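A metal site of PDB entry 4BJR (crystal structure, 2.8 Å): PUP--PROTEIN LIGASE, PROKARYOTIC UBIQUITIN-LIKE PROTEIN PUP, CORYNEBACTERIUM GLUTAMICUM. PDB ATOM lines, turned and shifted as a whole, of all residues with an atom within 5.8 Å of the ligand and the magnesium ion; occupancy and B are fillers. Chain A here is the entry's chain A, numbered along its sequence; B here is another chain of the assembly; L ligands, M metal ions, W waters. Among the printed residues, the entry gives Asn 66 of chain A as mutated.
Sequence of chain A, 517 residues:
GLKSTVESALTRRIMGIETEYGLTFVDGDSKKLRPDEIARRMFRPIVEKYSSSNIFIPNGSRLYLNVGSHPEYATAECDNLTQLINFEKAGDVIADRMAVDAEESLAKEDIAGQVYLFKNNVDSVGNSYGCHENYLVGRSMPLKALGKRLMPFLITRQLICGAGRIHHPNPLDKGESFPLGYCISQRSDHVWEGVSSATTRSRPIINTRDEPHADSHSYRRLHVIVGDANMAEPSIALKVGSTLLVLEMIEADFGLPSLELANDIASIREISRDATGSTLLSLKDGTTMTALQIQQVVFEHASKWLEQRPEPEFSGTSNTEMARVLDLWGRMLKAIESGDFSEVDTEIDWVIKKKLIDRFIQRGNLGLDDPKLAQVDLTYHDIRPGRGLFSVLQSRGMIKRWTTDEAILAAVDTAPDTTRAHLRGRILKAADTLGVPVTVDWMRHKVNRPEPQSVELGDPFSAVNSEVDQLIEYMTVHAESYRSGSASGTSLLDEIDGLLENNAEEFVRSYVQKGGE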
ATOM      1  N   ILE A  14      19.166  -5.121  17.123  1.00  0.00           N
ATOM      2  CA  ILE A  14      20.161  -5.432  16.108  1.00  0.00           C
ATOM      3  C   ILE A  14      20.175  -6.926  15.810  1.00  0.00           C
ATOM      4  O   ILE A  14      20.270  -7.748  16.712  1.00  0.00           O
ATOM      5  CB  ILE A  14      21.552  -5.004  16.541  1.00  0.00           C
ATOM      6  CG1 ILE A  14      21.602  -3.501  16.722  1.00  0.00           C
ATOM      7  CG2 ILE A  14      22.574  -5.443  15.526  1.00  0.00           C
ATOM      8  CD1 ILE A  14      21.510  -2.760  15.455  1.00  0.00           C
ATOM      9  N   MET A  15      20.069  -7.261  14.538  1.00  0.00           N
ATOM     10  CA  MET A  15      20.141  -8.649  14.119  1.00  0.00           C
ATOM     11  C   MET A  15      21.004  -8.826  12.890  1.00  0.00           C
ATOM     12  O   MET A  15      21.060  -7.956  12.031  1.00  0.00           O
ATOM     13  CB  MET A  15      18.746  -9.202  13.861  1.00  0.00           C
ATOM     14  CG  MET A  15      17.846  -8.290  13.088  1.00  0.00           C
ATOM     15  SD  MET A  15      16.247  -9.030  12.863  1.00  0.00           S
ATOM     16  CE  MET A  15      15.262  -7.575  12.656  1.00  0.00           C
ATOM     17  N   GLY A  16      21.724  -9.940  12.814  1.00  0.00           N
ATOM     18  CA  GLY A  16      22.508 -10.242  11.647  1.00  0.00           C
ATOM     19  C   GLY A  16      22.464 -11.701  11.260  1.00  0.00           C
ATOM     20  O   GLY A  16      22.127 -12.546  12.072  1.00  0.00           O
ATOM     21  N   ILE A  17      22.808 -11.990  10.010  1.00  0.00           N
ATOM     22  CA  ILE A  17      22.854 -13.368   9.534  1.00  0.00           C
ATOM     23  C   ILE A  17      24.208 -13.725   8.960  1.00  0.00           C
ATOM     24  O   ILE A  17      24.786 -12.981   8.193  1.00  0.00           O
ATOM     25  CB  ILE A  17      21.790 -13.612   8.468  1.00  0.00           C
ATOM     26  CG1 ILE A  17      20.401 -13.441   9.069  1.00  0.00           C
ATOM     27  CG2 ILE A  17      21.908 -14.993   7.892  1.00  0.00           C
ATOM     28  CD1 ILE A  17      19.950 -14.578   9.890  1.00  0.00           C
ATOM     29  N   GLU A  18      24.704 -14.893   9.344  1.00  0.00           N
ATOM     30  CA  GLU A  18      25.929 -15.420   8.793  1.00  0.00           C
ATOM     31  C   GLU A  18      25.617 -16.563   7.855  1.00  0.00           C
ATOM     32  O   GLU A  18      25.105 -17.585   8.285  1.00  0.00           O
ATOM     33  CB  GLU A  18      26.859 -15.901   9.906  1.00  0.00           C
ATOM     34  CG  GLU A  18      27.563 -14.821  10.682  1.00  0.00           C
ATOM     35  CD  GLU A  18      28.339 -15.388  11.845  1.00  0.00           C
ATOM     36  OE1 GLU A  18      29.142 -16.305  11.627  1.00  0.00           O
ATOM     37  OE2 GLU A  18      28.162 -14.907  12.970  1.00  0.00           O
ATOM     38  N   PHE A  56      35.505  -6.179   4.384  1.00  0.00           N
ATOM     39  CA  PHE A  56      34.210  -5.550   4.592  1.00  0.00           C
ATOM     40  C   PHE A  56      33.858  -4.741   3.359  1.00  0.00           C
ATOM     41  O   PHE A  56      34.617  -3.896   2.928  1.00  0.00           O
ATOM     42  CB  PHE A  56      34.247  -4.652   5.814  1.00  0.00           C
ATOM     43  CG  PHE A  56      33.923  -5.342   7.102  1.00  0.00           C
ATOM     44  CD1 PHE A  56      34.895  -6.022   7.801  1.00  0.00           C
ATOM     45  CD2 PHE A  56      32.661  -5.288   7.623  1.00  0.00           C
ATOM     46  CE1 PHE A  56      34.610  -6.642   8.974  1.00  0.00           C
ATOM     47  CE2 PHE A  56      32.372  -5.903   8.803  1.00  0.00           C
ATOM     48  CZ  PHE A  56      33.347  -6.578   9.485  1.00  0.00           C
ATOM     49  N   ARG A  62      30.232  -8.254   5.965  1.00  0.00           N
ATOM     50  CA  ARG A  62      31.532  -8.881   5.940  1.00  0.00           C
ATOM     51  C   ARG A  62      31.541 -10.036   4.958  1.00  0.00           C
ATOM     52  O   ARG A  62      30.678 -10.883   4.985  1.00  0.00           O
ATOM     53  CB  ARG A  62      31.917  -9.345   7.335  1.00  0.00           C
ATOM     54  CG  ARG A  62      33.294  -9.935   7.450  1.00  0.00           C
ATOM     55  CD  ARG A  62      33.581 -10.353   8.872  1.00  0.00           C
ATOM     56  NE  ARG A  62      34.867 -11.016   8.992  1.00  0.00           N
ATOM     57  CZ  ARG A  62      35.086 -12.066   9.764  1.00  0.00           C
ATOM     58  NH1 ARG A  62      34.109 -12.589  10.481  1.00  0.00           N
ATOM     59  NH2 ARG A  62      36.292 -12.615   9.816  1.00  0.00           N
ATOM     60  N   TYR A  64      34.010 -13.074   3.436  1.00  0.00           N
ATOM     61  CA  TYR A  64      35.289 -13.731   3.623  1.00  0.00           C
ATOM     62  C   TYR A  64      35.326 -15.198   3.269  1.00  0.00           C
ATOM     63  O   TYR A  64      34.312 -15.820   3.076  1.00  0.00           O
ATOM     64  CB  TYR A  64      35.781 -13.572   5.062  1.00  0.00           C
ATOM     65  CG  TYR A  64      34.924 -14.154   6.160  1.00  0.00           C
ATOM     66  CD1 TYR A  64      33.715 -13.594   6.491  1.00  0.00           C
ATOM     67  CD2 TYR A  64      35.371 -15.233   6.900  1.00  0.00           C
ATOM     68  CE1 TYR A  64      32.963 -14.111   7.524  1.00  0.00           C
ATOM     69  CE2 TYR A  64      34.622 -15.746   7.916  1.00  0.00           C
ATOM     70  CZ  TYR A  64      33.421 -15.188   8.225  1.00  0.00           C
ATOM     71  OH  TYR A  64      32.668 -15.695   9.247  1.00  0.00           O
ATOM     72  N   ASN A  66      36.066 -18.853   4.355  1.00  0.00           N
ATOM     73  CA  ASN A  66      36.025 -19.642   5.576  1.00  0.00           C
ATOM     74  C   ASN A  66      37.170 -20.607   5.728  1.00  0.00           C
ATOM     75  O   ASN A  66      37.844 -20.963   4.780  1.00  0.00           O
ATOM     76  CB  ASN A  66      34.729 -20.439   5.627  1.00  0.00           C
ATOM     77  CG  ASN A  66      34.021 -20.311   6.931  1.00  0.00           C
ATOM     78  OD1 ASN A  66      34.452 -19.576   7.810  1.00  0.00           O
ATOM     79  ND2 ASN A  66      32.930 -21.033   7.067  1.00  0.00           N
ATOM     80  N   GLU A  72      31.733 -17.036   2.821  1.00  0.00           N
ATOM     81  CA  GLU A  72      30.828 -16.652   3.890  1.00  0.00           C
ATOM     82  C   GLU A  72      30.474 -15.177   3.821  1.00  0.00           C
ATOM     83  O   GLU A  72      31.320 -14.311   3.674  1.00  0.00           O
ATOM     84  CB  GLU A  72      31.437 -16.975   5.245  1.00  0.00           C
ATOM     85  CG  GLU A  72      30.552 -16.572   6.402  1.00  0.00           C
ATOM     86  CD  GLU A  72      30.888 -17.282   7.686  1.00  0.00           C
ATOM     87  OE1 GLU A  72      31.527 -18.350   7.633  1.00  0.00           O
ATOM     88  OE2 GLU A  72      30.529 -16.761   8.758  1.00  0.00           O
ATOM     89  N   ALA A  74      28.378 -12.288   5.950  1.00  0.00           N
ATOM     90  CA  ALA A  74      27.746 -11.911   7.197  1.00  0.00           C
ATOM     91  C   ALA A  74      27.102 -10.566   7.005  1.00  0.00           C
ATOM     92  O   ALA A  74      27.761  -9.604   6.641  1.00  0.00           O
ATOM     93  CB  ALA A  74      28.742 -11.872   8.314  1.00  0.00           C
ATOM     94  N   THR A  75      25.805 -10.489   7.251  1.00  0.00           N
ATOM     95  CA  THR A  75      25.079  -9.280   6.962  1.00  0.00           C
ATOM     96  C   THR A  75      25.503  -8.154   7.841  1.00  0.00           C
ATOM     97  O   THR A  75      25.942  -8.348   8.960  1.00  0.00           O
ATOM     98  CB  THR A  75      23.574  -9.456   7.134  1.00  0.00           C
ATOM     99  OG1 THR A  75      23.286  -9.685   8.521  1.00  0.00           O
ATOM    100  CG2 THR A  75      23.090 -10.610   6.332  1.00  0.00           C
ATOM    101  N   ALA A  76      25.354  -6.954   7.314  1.00  0.00           N
ATOM    102  CA  ALA A  76      25.503  -5.763   8.096  1.00  0.00           C
ATOM    103  C   ALA A  76      24.415  -5.751   9.140  1.00  0.00           C
ATOM    104  O   ALA A  76      23.397  -6.400   8.970  1.00  0.00           O
ATOM    105  CB  ALA A  76      25.418  -4.552   7.221  1.00  0.00           C
ATOM    106  N   GLU A  77      24.649  -5.044  10.231  1.00  0.00           N
ATOM    107  CA  GLU A  77      23.666  -4.974  11.294  1.00  0.00           C
ATOM    108  C   GLU A  77      22.378  -4.377  10.775  1.00  0.00           C
ATOM    109  O   GLU A  77      22.382  -3.356  10.092  1.00  0.00           O
ATOM    110  CB  GLU A  77      24.182  -4.137  12.457  1.00  0.00           C
ATOM    111  CG  GLU A  77      25.525  -4.568  12.966  1.00  0.00           C
ATOM    112  CD  GLU A  77      26.652  -3.796  12.335  1.00  0.00           C
ATOM    113  OE1 GLU A  77      26.636  -3.610  11.115  1.00  0.00           O
ATOM    114  OE2 GLU A  77      27.573  -3.392  13.063  1.00  0.00           O
ATOM    115  N   CYS A  78      21.271  -5.031  11.082  1.00  0.00           N
ATOM    116  CA  CYS A  78      19.956  -4.582  10.668  1.00  0.00           C
ATOM    117  C   CYS A  78      19.032  -4.498  11.880  1.00  0.00           C
ATOM    118  O   CYS A  78      19.080  -5.347  12.760  1.00  0.00           O
ATOM    119  CB  CYS A  78      19.380  -5.529   9.611  1.00  0.00           C
ATOM    120  SG  CYS A  78      20.282  -5.608   8.074  1.00  0.00           S
ATOM    121  N   ASN A 134      22.143 -13.979  14.570  1.00  0.00           N
ATOM    122  CA  ASN A 134      22.627 -13.153  15.675  1.00  0.00           C
ATOM    123  C   ASN A 134      21.616 -12.125  16.136  1.00  0.00           C
ATOM    124  O   ASN A 134      21.158 -11.310  15.343  1.00  0.00           O
ATOM    125  CB  ASN A 134      23.925 -12.462  15.267  1.00  0.00           C
ATOM    126  CG  ASN A 134      24.961 -13.433  14.801  1.00  0.00           C
ATOM    127  OD1 ASN A 134      25.789 -13.877  15.580  1.00  0.00           O
ATOM    128  ND2 ASN A 134      24.925 -13.768  13.531  1.00  0.00           N
ATOM    129  N   TYR A 135      21.302 -12.135  17.425  1.00  0.00           N
ATOM    130  CA  TYR A 135      20.357 -11.178  17.998  1.00  0.00           C
ATOM    131  C   TYR A 135      20.935 -10.400  19.167  1.00  0.00           C
ATOM    132  O   TYR A 135      21.469 -10.980  20.099  1.00  0.00           O
ATOM    133  CB  TYR A 135      19.102 -11.904  18.468  1.00  0.00           C
ATOM    134  CG  TYR A 135      18.445 -12.792  17.439  1.00  0.00           C
ATOM    135  CD1 TYR A 135      17.485 -12.292  16.578  1.00  0.00           C
ATOM    136  CD2 TYR A 135      18.772 -14.122  17.354  1.00  0.00           C
ATOM    137  CE1 TYR A 135      16.889 -13.107  15.646  1.00  0.00           C
ATOM    138  CE2 TYR A 135      18.183 -14.940  16.429  1.00  0.00           C
ATOM    139  CZ  TYR A 135      17.247 -14.430  15.576  1.00  0.00           C
ATOM    140  OH  TYR A 135      16.663 -15.254  14.644  1.00  0.00           O
ATOM    141  N   LEU A 136      20.824  -9.083  19.136  1.00  0.00           N
ATOM    142  CA  LEU A 136      21.244  -8.269  20.255  1.00  0.00           C
ATOM    143  C   LEU A 136      20.329  -8.456  21.435  1.00  0.00           C
ATOM    144  O   LEU A 136      19.114  -8.487  21.273  1.00  0.00           O
ATOM    145  CB  LEU A 136      21.303  -6.788  19.869  1.00  0.00           C
ATOM    146  CG  LEU A 136      21.559  -5.782  20.987  1.00  0.00           C
ATOM    147  CD1 LEU A 136      22.526  -4.733  20.539  1.00  0.00           C
ATOM    148  CD2 LEU A 136      20.269  -5.136  21.413  1.00  0.00           C
ATOM    149  N   ASP A 210      30.000 -15.098  23.417  1.00  0.00           N
ATOM    150  CA  ASP A 210      30.903 -14.520  22.431  1.00  0.00           C
ATOM    151  C   ASP A 210      30.791 -13.018  22.365  1.00  0.00           C
ATOM    152  O   ASP A 210      29.806 -12.460  22.822  1.00  0.00           O
ATOM    153  CB  ASP A 210      30.658 -15.113  21.044  1.00  0.00           C
ATOM    154  CG  ASP A 210      31.878 -15.050  20.172  1.00  0.00           C
ATOM    155  OD1 ASP A 210      32.807 -14.333  20.540  1.00  0.00           O
ATOM    156  OD2 ASP A 210      31.899 -15.688  19.115  1.00  0.00           O
ATOM    157  N   GLU A 211      31.808 -12.375  21.825  1.00  0.00           N
ATOM    158  CA  GLU A 211      31.869 -10.923  21.832  1.00  0.00           C
ATOM    159  C   GLU A 211      30.670 -10.272  21.188  1.00  0.00           C
ATOM    160  O   GLU A 211      30.301 -10.608  20.072  1.00  0.00           O
ATOM    161  CB  GLU A 211      33.127 -10.438  21.130  1.00  0.00           C
ATOM    162  CG  GLU A 211      33.637 -11.311  20.030  1.00  0.00           C
ATOM    163  CD  GLU A 211      34.967 -10.830  19.487  1.00  0.00           C
ATOM    164  OE1 GLU A 211      35.266  -9.631  19.618  1.00  0.00           O
ATOM    165  OE2 GLU A 211      35.710 -11.653  18.927  1.00  0.00           O
ATOM    166  N   PRO A 212      30.068  -9.303  21.891  1.00  0.00           N
ATOM    167  CA  PRO A 212      28.835  -8.615  21.539  1.00  0.00           C
ATOM    168  C   PRO A 212      28.951  -7.775  20.291  1.00  0.00           C
ATOM    169  O   PRO A 212      27.954  -7.597  19.613  1.00  0.00           O
ATOM    170  CB  PRO A 212      28.572  -7.738  22.759  1.00  0.00           C
ATOM    171  CG  PRO A 212      29.857  -7.596  23.398  1.00  0.00           C
ATOM    172  CD  PRO A 212      30.538  -8.884  23.212  1.00  0.00           C
ATOM    173  N   HIS A 213      30.142  -7.231  20.037  1.00  0.00           N
ATOM    174  CA  HIS A 213      30.350  -6.274  18.958  1.00  0.00           C
ATOM    175  C   HIS A 213      29.537  -5.026  19.259  1.00  0.00           C
ATOM    176  O   HIS A 213      29.132  -4.274  18.376  1.00  0.00           O
ATOM    177  CB  HIS A 213      29.991  -6.876  17.593  1.00  0.00           C
ATOM    178  CG  HIS A 213      30.904  -7.986  17.170  1.00  0.00           C
ATOM    179  ND1 HIS A 213      30.455  -9.078  16.458  1.00  0.00           N
ATOM    180  CD2 HIS A 213      32.235  -8.154  17.321  1.00  0.00           C
ATOM    181  CE1 HIS A 213      31.466  -9.885  16.219  1.00  0.00           C
ATOM    182  NE2 HIS A 213      32.566  -9.347  16.732  1.00  0.00           N
ATOM    183  N   ALA A 214      29.286  -4.858  20.548  1.00  0.00           N
ATOM    184  CA  ALA A 214      28.626  -3.715  21.111  1.00  0.00           C
ATOM    185  C   ALA A 214      29.218  -3.460  22.485  1.00  0.00           C
ATOM    186  O   ALA A 214      29.979  -4.286  22.977  1.00  0.00           O
ATOM    187  CB  ALA A 214      27.152  -3.924  21.198  1.00  0.00           C
ATOM    188  N   ARG A 220      24.726  -7.955  25.043  1.00  0.00           N
ATOM    189  CA  ARG A 220      25.278  -9.236  24.625  1.00  0.00           C
ATOM    190  C   ARG A 220      24.778  -9.592  23.240  1.00  0.00           C
ATOM    191  O   ARG A 220      23.793  -9.050  22.766  1.00  0.00           O
ATOM    192  CB  ARG A 220      24.897 -10.357  25.586  1.00  0.00           C
ATOM    193  CG  ARG A 220      25.606 -10.325  26.895  1.00  0.00           C
ATOM    194  CD  ARG A 220      25.249 -11.550  27.679  1.00  0.00           C
ATOM    195  NE  ARG A 220      25.702 -11.480  29.052  1.00  0.00           N
ATOM    196  CZ  ARG A 220      26.841 -11.997  29.485  1.00  0.00           C
ATOM    197  NH1 ARG A 220      27.646 -12.621  28.647  1.00  0.00           N
ATOM    198  NH2 ARG A 220      27.174 -11.889  30.757  1.00  0.00           N
ATOM    199  N   ARG A 221      25.480 -10.521  22.598  1.00  0.00           N
ATOM    200  CA  ARG A 221      25.056 -11.042  21.311  1.00  0.00           C
ATOM    201  C   ARG A 221      24.649 -12.489  21.444  1.00  0.00           C
ATOM    202  O   ARG A 221      25.387 -13.307  21.975  1.00  0.00           O
ATOM    203  CB  ARG A 221      26.180 -10.900  20.286  1.00  0.00           C
ATOM    204  CG  ARG A 221      25.759 -11.093  18.866  1.00  0.00           C
ATOM    205  CD  ARG A 221      26.892 -10.833  17.890  1.00  0.00           C
ATOM    206  NE  ARG A 221      28.193 -11.176  18.441  1.00  0.00           N
ATOM    207  CZ  ARG A 221      28.957 -12.155  17.995  1.00  0.00           C
ATOM    208  NH1 ARG A 221      28.547 -12.904  16.990  1.00  0.00           N
ATOM    209  NH2 ARG A 221      30.125 -12.382  18.545  1.00  0.00           N
ATOM    210  N   HIS A 223      23.808 -16.004  19.779  1.00  0.00           N
ATOM    211  CA  HIS A 223      24.206 -16.723  18.583  1.00  0.00           C
ATOM    212  C   HIS A 223      23.446 -18.027  18.463  1.00  0.00           C
ATOM    213  O   HIS A 223      23.479 -18.861  19.350  1.00  0.00           O
ATOM    214  CB  HIS A 223      25.706 -17.003  18.616  1.00  0.00           C
ATOM    215  CG  HIS A 223      26.278 -17.462  17.313  1.00  0.00           C
ATOM    216  ND1 HIS A 223      26.357 -16.641  16.211  1.00  0.00           N
ATOM    217  CD2 HIS A 223      26.789 -18.654  16.937  1.00  0.00           C
ATOM    218  CE1 HIS A 223      26.895 -17.309  15.214  1.00  0.00           C
ATOM    219  NE2 HIS A 223      27.170 -18.534  15.623  1.00  0.00           N
ATOM    220  N   ARG A 420      24.298   1.094  12.753  1.00  0.00           N
ATOM    221  CA  ARG A 420      25.692   1.518  12.719  1.00  0.00           C
ATOM    222  C   ARG A 420      26.377   1.242  11.399  1.00  0.00           C
ATOM    223  O   ARG A 420      27.312   1.947  11.019  1.00  0.00           O
ATOM    224  CB  ARG A 420      26.450   0.820  13.853  1.00  0.00           C
ATOM    225  CG  ARG A 420      27.937   0.678  13.643  1.00  0.00           C
ATOM    226  CD  ARG A 420      28.583   0.082  14.850  1.00  0.00           C
ATOM    227  NE  ARG A 420      28.269  -1.322  15.037  1.00  0.00           N
ATOM    228  CZ  ARG A 420      28.610  -2.010  16.121  1.00  0.00           C
ATOM    229  NH1 ARG A 420      29.276  -1.417  17.094  1.00  0.00           N
ATOM    230  NH2 ARG A 420      28.298  -3.286  16.235  1.00  0.00           N
ATOM    231  N   TRP A 442      33.667  -4.646  13.037  1.00  0.00           N
ATOM    232  CA  TRP A 442      32.306  -4.353  13.437  1.00  0.00           C
ATOM    233  C   TRP A 442      32.294  -3.124  14.333  1.00  0.00           C
ATOM    234  O   TRP A 442      31.556  -2.186  14.104  1.00  0.00           O
ATOM    235  CB  TRP A 442      31.666  -5.533  14.153  1.00  0.00           C
ATOM    236  CG  TRP A 442      31.481  -6.729  13.290  1.00  0.00           C
ATOM    237  CD1 TRP A 442      32.139  -7.907  13.397  1.00  0.00           C
ATOM    238  CD2 TRP A 442      30.594  -6.857  12.192  1.00  0.00           C
ATOM    239  NE1 TRP A 442      31.709  -8.773  12.427  1.00  0.00           N
ATOM    240  CE2 TRP A 442      30.761  -8.147  11.672  1.00  0.00           C
ATOM    241  CE3 TRP A 442      29.665  -6.011  11.597  1.00  0.00           C
ATOM    242  CZ2 TRP A 442      30.033  -8.604  10.591  1.00  0.00           C
ATOM    243  CZ3 TRP A 442      28.944  -6.470  10.523  1.00  0.00           C
ATOM    244  CH2 TRP A 442      29.133  -7.754  10.027  1.00  0.00           C
ATOM    245  N   PRO A 460      25.725   0.089  18.167  1.00  0.00           N
ATOM    246  CA  PRO A 460      25.217  -0.494  16.926  1.00  0.00           C
ATOM    247  C   PRO A 460      24.028   0.269  16.383  1.00  0.00           C
ATOM    248  O   PRO A 460      23.825   0.313  15.181  1.00  0.00           O
ATOM    249  CB  PRO A 460      24.832  -1.913  17.337  1.00  0.00           C
ATOM    250  CG  PRO A 460      24.643  -1.855  18.771  1.00  0.00           C
ATOM    251  CD  PRO A 460      25.599  -0.863  19.283  1.00  0.00           C
ATOM    252  N   GLU B 517      33.044 -24.054  10.844  1.00  0.00           N
ATOM    253  CA  GLU B 517      32.733 -23.575  12.201  1.00  0.00           C
ATOM    254  C   GLU B 517      31.806 -24.499  12.972  1.00  0.00           C
ATOM    255  O   GLU B 517      31.996 -24.738  14.161  1.00  0.00           O
ATOM    256  CB  GLU B 517      32.138 -22.160  12.145  1.00  0.00           C
ATOM    257  CG  GLU B 517      31.559 -21.709  13.482  1.00  0.00           C
ATOM    258  CD  GLU B 517      32.586 -21.524  14.592  1.00  0.00           C
ATOM    259  OE1 GLU B 517      33.675 -20.951  14.347  1.00  0.00           O
ATOM    260  OE2 GLU B 517      32.324 -22.010  15.717  1.00  0.00           O
HETATM  261  P1  LIG L   1      34.679 -15.160  13.679  1.00  0.00           P
HETATM  262  O1  LIG L   1      35.025 -14.524  12.365  1.00  0.00           O
HETATM  263  O2  LIG L   1      34.066 -16.527  13.551  1.00  0.00           O
HETATM  264  O3  LIG L   1      35.734 -15.045  14.736  1.00  0.00           O
HETATM  265  P2  LIG L   1      32.006 -14.375  13.779  1.00  0.00           P
HETATM  266  O4  LIG L   1      31.952 -15.350  12.632  1.00  0.00           O
HETATM  267  O5  LIG L   1      31.177 -14.621  15.011  1.00  0.00           O
HETATM  268  O6  LIG L   1      33.524 -14.223  14.264  1.00  0.00           O
HETATM  269  P3  LIG L   1      31.023 -12.541  11.880  1.00  0.00           P
HETATM  270  O7  LIG L   1      31.491 -11.175  11.529  1.00  0.00           O
HETATM  271  O8  LIG L   1      31.181 -13.652  10.898  1.00  0.00           O
HETATM  272  O9  LIG L   1      31.714 -12.882  13.279  1.00  0.00           O
HETATM  273  O10 LIG L   1      29.485 -12.458  12.308  1.00  0.00           O
HETATM  274  C1  LIG L   1      29.004 -11.221  12.785  1.00  0.00           C
HETATM  275  C2  LIG L   1      27.494 -11.155  12.759  1.00  0.00           C
HETATM  276  O11 LIG L   1      27.055 -10.478  13.937  1.00  0.00           O
HETATM  277  C3  LIG L   1      27.036 -10.332  11.592  1.00  0.00           C
HETATM  278  O12 LIG L   1      25.963 -11.027  10.969  1.00  0.00           O
HETATM  279  C4  LIG L   1      26.504  -9.052  12.178  1.00  0.00           C
HETATM  280  O13 LIG L   1      25.363  -8.669  11.440  1.00  0.00           O
HETATM  281  C5  LIG L   1      26.151  -9.448  13.585  1.00  0.00           C
HETATM  282  N1  LIG L   1      26.330  -8.351  14.550  1.00  0.00           N
HETATM  283  C6  LIG L   1      27.289  -7.423  14.545  1.00  0.00           C
HETATM  284  N2  LIG L   1      27.149  -6.579  15.589  1.00  0.00           N
HETATM  285  C7  LIG L   1      26.088  -6.980  16.286  1.00  0.00           C
HETATM  286  C8  LIG L   1      25.378  -6.542  17.501  1.00  0.00           C
HETATM  287  N3  LIG L   1      25.783  -5.473  18.205  1.00  0.00           N
HETATM  288  N4  LIG L   1      24.296  -7.254  17.877  1.00  0.00           N
HETATM  289  C9  LIG L   1      23.865  -8.310  17.189  1.00  0.00           C
HETATM  290  N5  LIG L   1      24.462  -8.763  16.080  1.00  0.00           N
HETATM  291  C10 LIG L   1      25.545  -8.149  15.596  1.00  0.00           C
HETATM  292 MG    MG M   1      31.357 -15.781  10.779  1.00  0.00          MG
HETATM  293  O   HOH W   1      37.357 -13.975  12.033  1.00  0.00           O
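ND2 of Asn 134 lies within hydrogen-bond range of OE2 of Glu 18, 3.5 Å away.
The backbone carbonyl oxygen (O) of Arg 62 is in hydrogen-bond range of the backbone NH (N) of Ala 74.
The backbone carbonyl oxygen (O) of Gly 16 sits at hydrogen-bond distance from the backbone NH (N) of Asn 134 (2.9 Å).
The backbone carbonyl oxygen (O) of His 213 lies within hydrogen-bond range of the guanidinium group (NH2) of Arg 420 (2.5 Å).
The side-chain carboxylate (OE2) of Glu 77 lies within salt-bridge range of the guanidinium group (NE) of Arg 420.
N of Arg 420 lies within hydrogen-bond range of O of Pro 460 (2.6 Å).
NH1 of Arg 221 is in hydrogen-bond range of OD1 of Asn 134, 3.2 Å away.
OD1 of Asn 134 sits at hydrogen-bond distance from ND1 of His 223.
The magnesium ion is bound by O4 of the ligand (2.0 Å), OH of Tyr 64 (2.0 Å), O8 of the ligand (2.1 Å), OE2 of Glu 72 (2.4 Å) and OE1 of Glu 18 (2.4 Å).
The magnesium ion has five donor atoms within binding distance.
Three residues have an atom within 4 Å of the magnesium ion: Glu 18, Tyr 64 and Glu 72.
Water W1 lies within hydrogen-bond range of O1 of the ligand and NH2 of Arg 62.
Ile 14 touches the ligand (CG2 to N4, 3.4 Å).
Gly 16 touches the ligand (CA to O13, 3.3 Å).
Ala 74 touches the ligand (CB to O12, 3.9 Å).
C of Ala 76 touches O13 of the ligand, 3.8 Å away.
CG of Glu 77 touches N2 of the ligand (3.7 Å).
Asn 134 touches the ligand.
CB of Leu 136 touches N4 of the ligand (3.6 Å).
His 213 touches the ligand.
CB of Ala 214 touches N3 of the ligand (3.6 Å).
Arg 420 touches the ligand.
CB of Pro 460 touches N3 of the ligand (3.8 Å).
Hydrophobic or aromatic side chains within 4 Å of the ligand: Ile 14, Tyr 64, Ala 74, Leu 136, His 213, Ala 214, Trp 442 and Pro 460.
The backbone carbonyl oxygen (O) of Thr 75 lies within hydrogen-bond range of an oxygen (O13) of the ligand, 2.6 Å away.
NE1 of Trp 442 sits at hydrogen-bond distance from O7 of the ligand (2.6 Å).
NH1 of Arg 62 is in salt-bridge range of O1 of the ligand (2.9 Å).
The backbone carbonyl oxygen (O) of Pro 212 is in hydrogen-bond range of a nitrogen (N3) of the ligand (3.3 Å).
O12 of the ligand lies within hydrogen-bond range of N of Ile 17, 3.4 Å away.
The guanidinium group of Arg 221 is in salt-bridge range of an oxygen (O5) of the ligand (3.7 Å).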
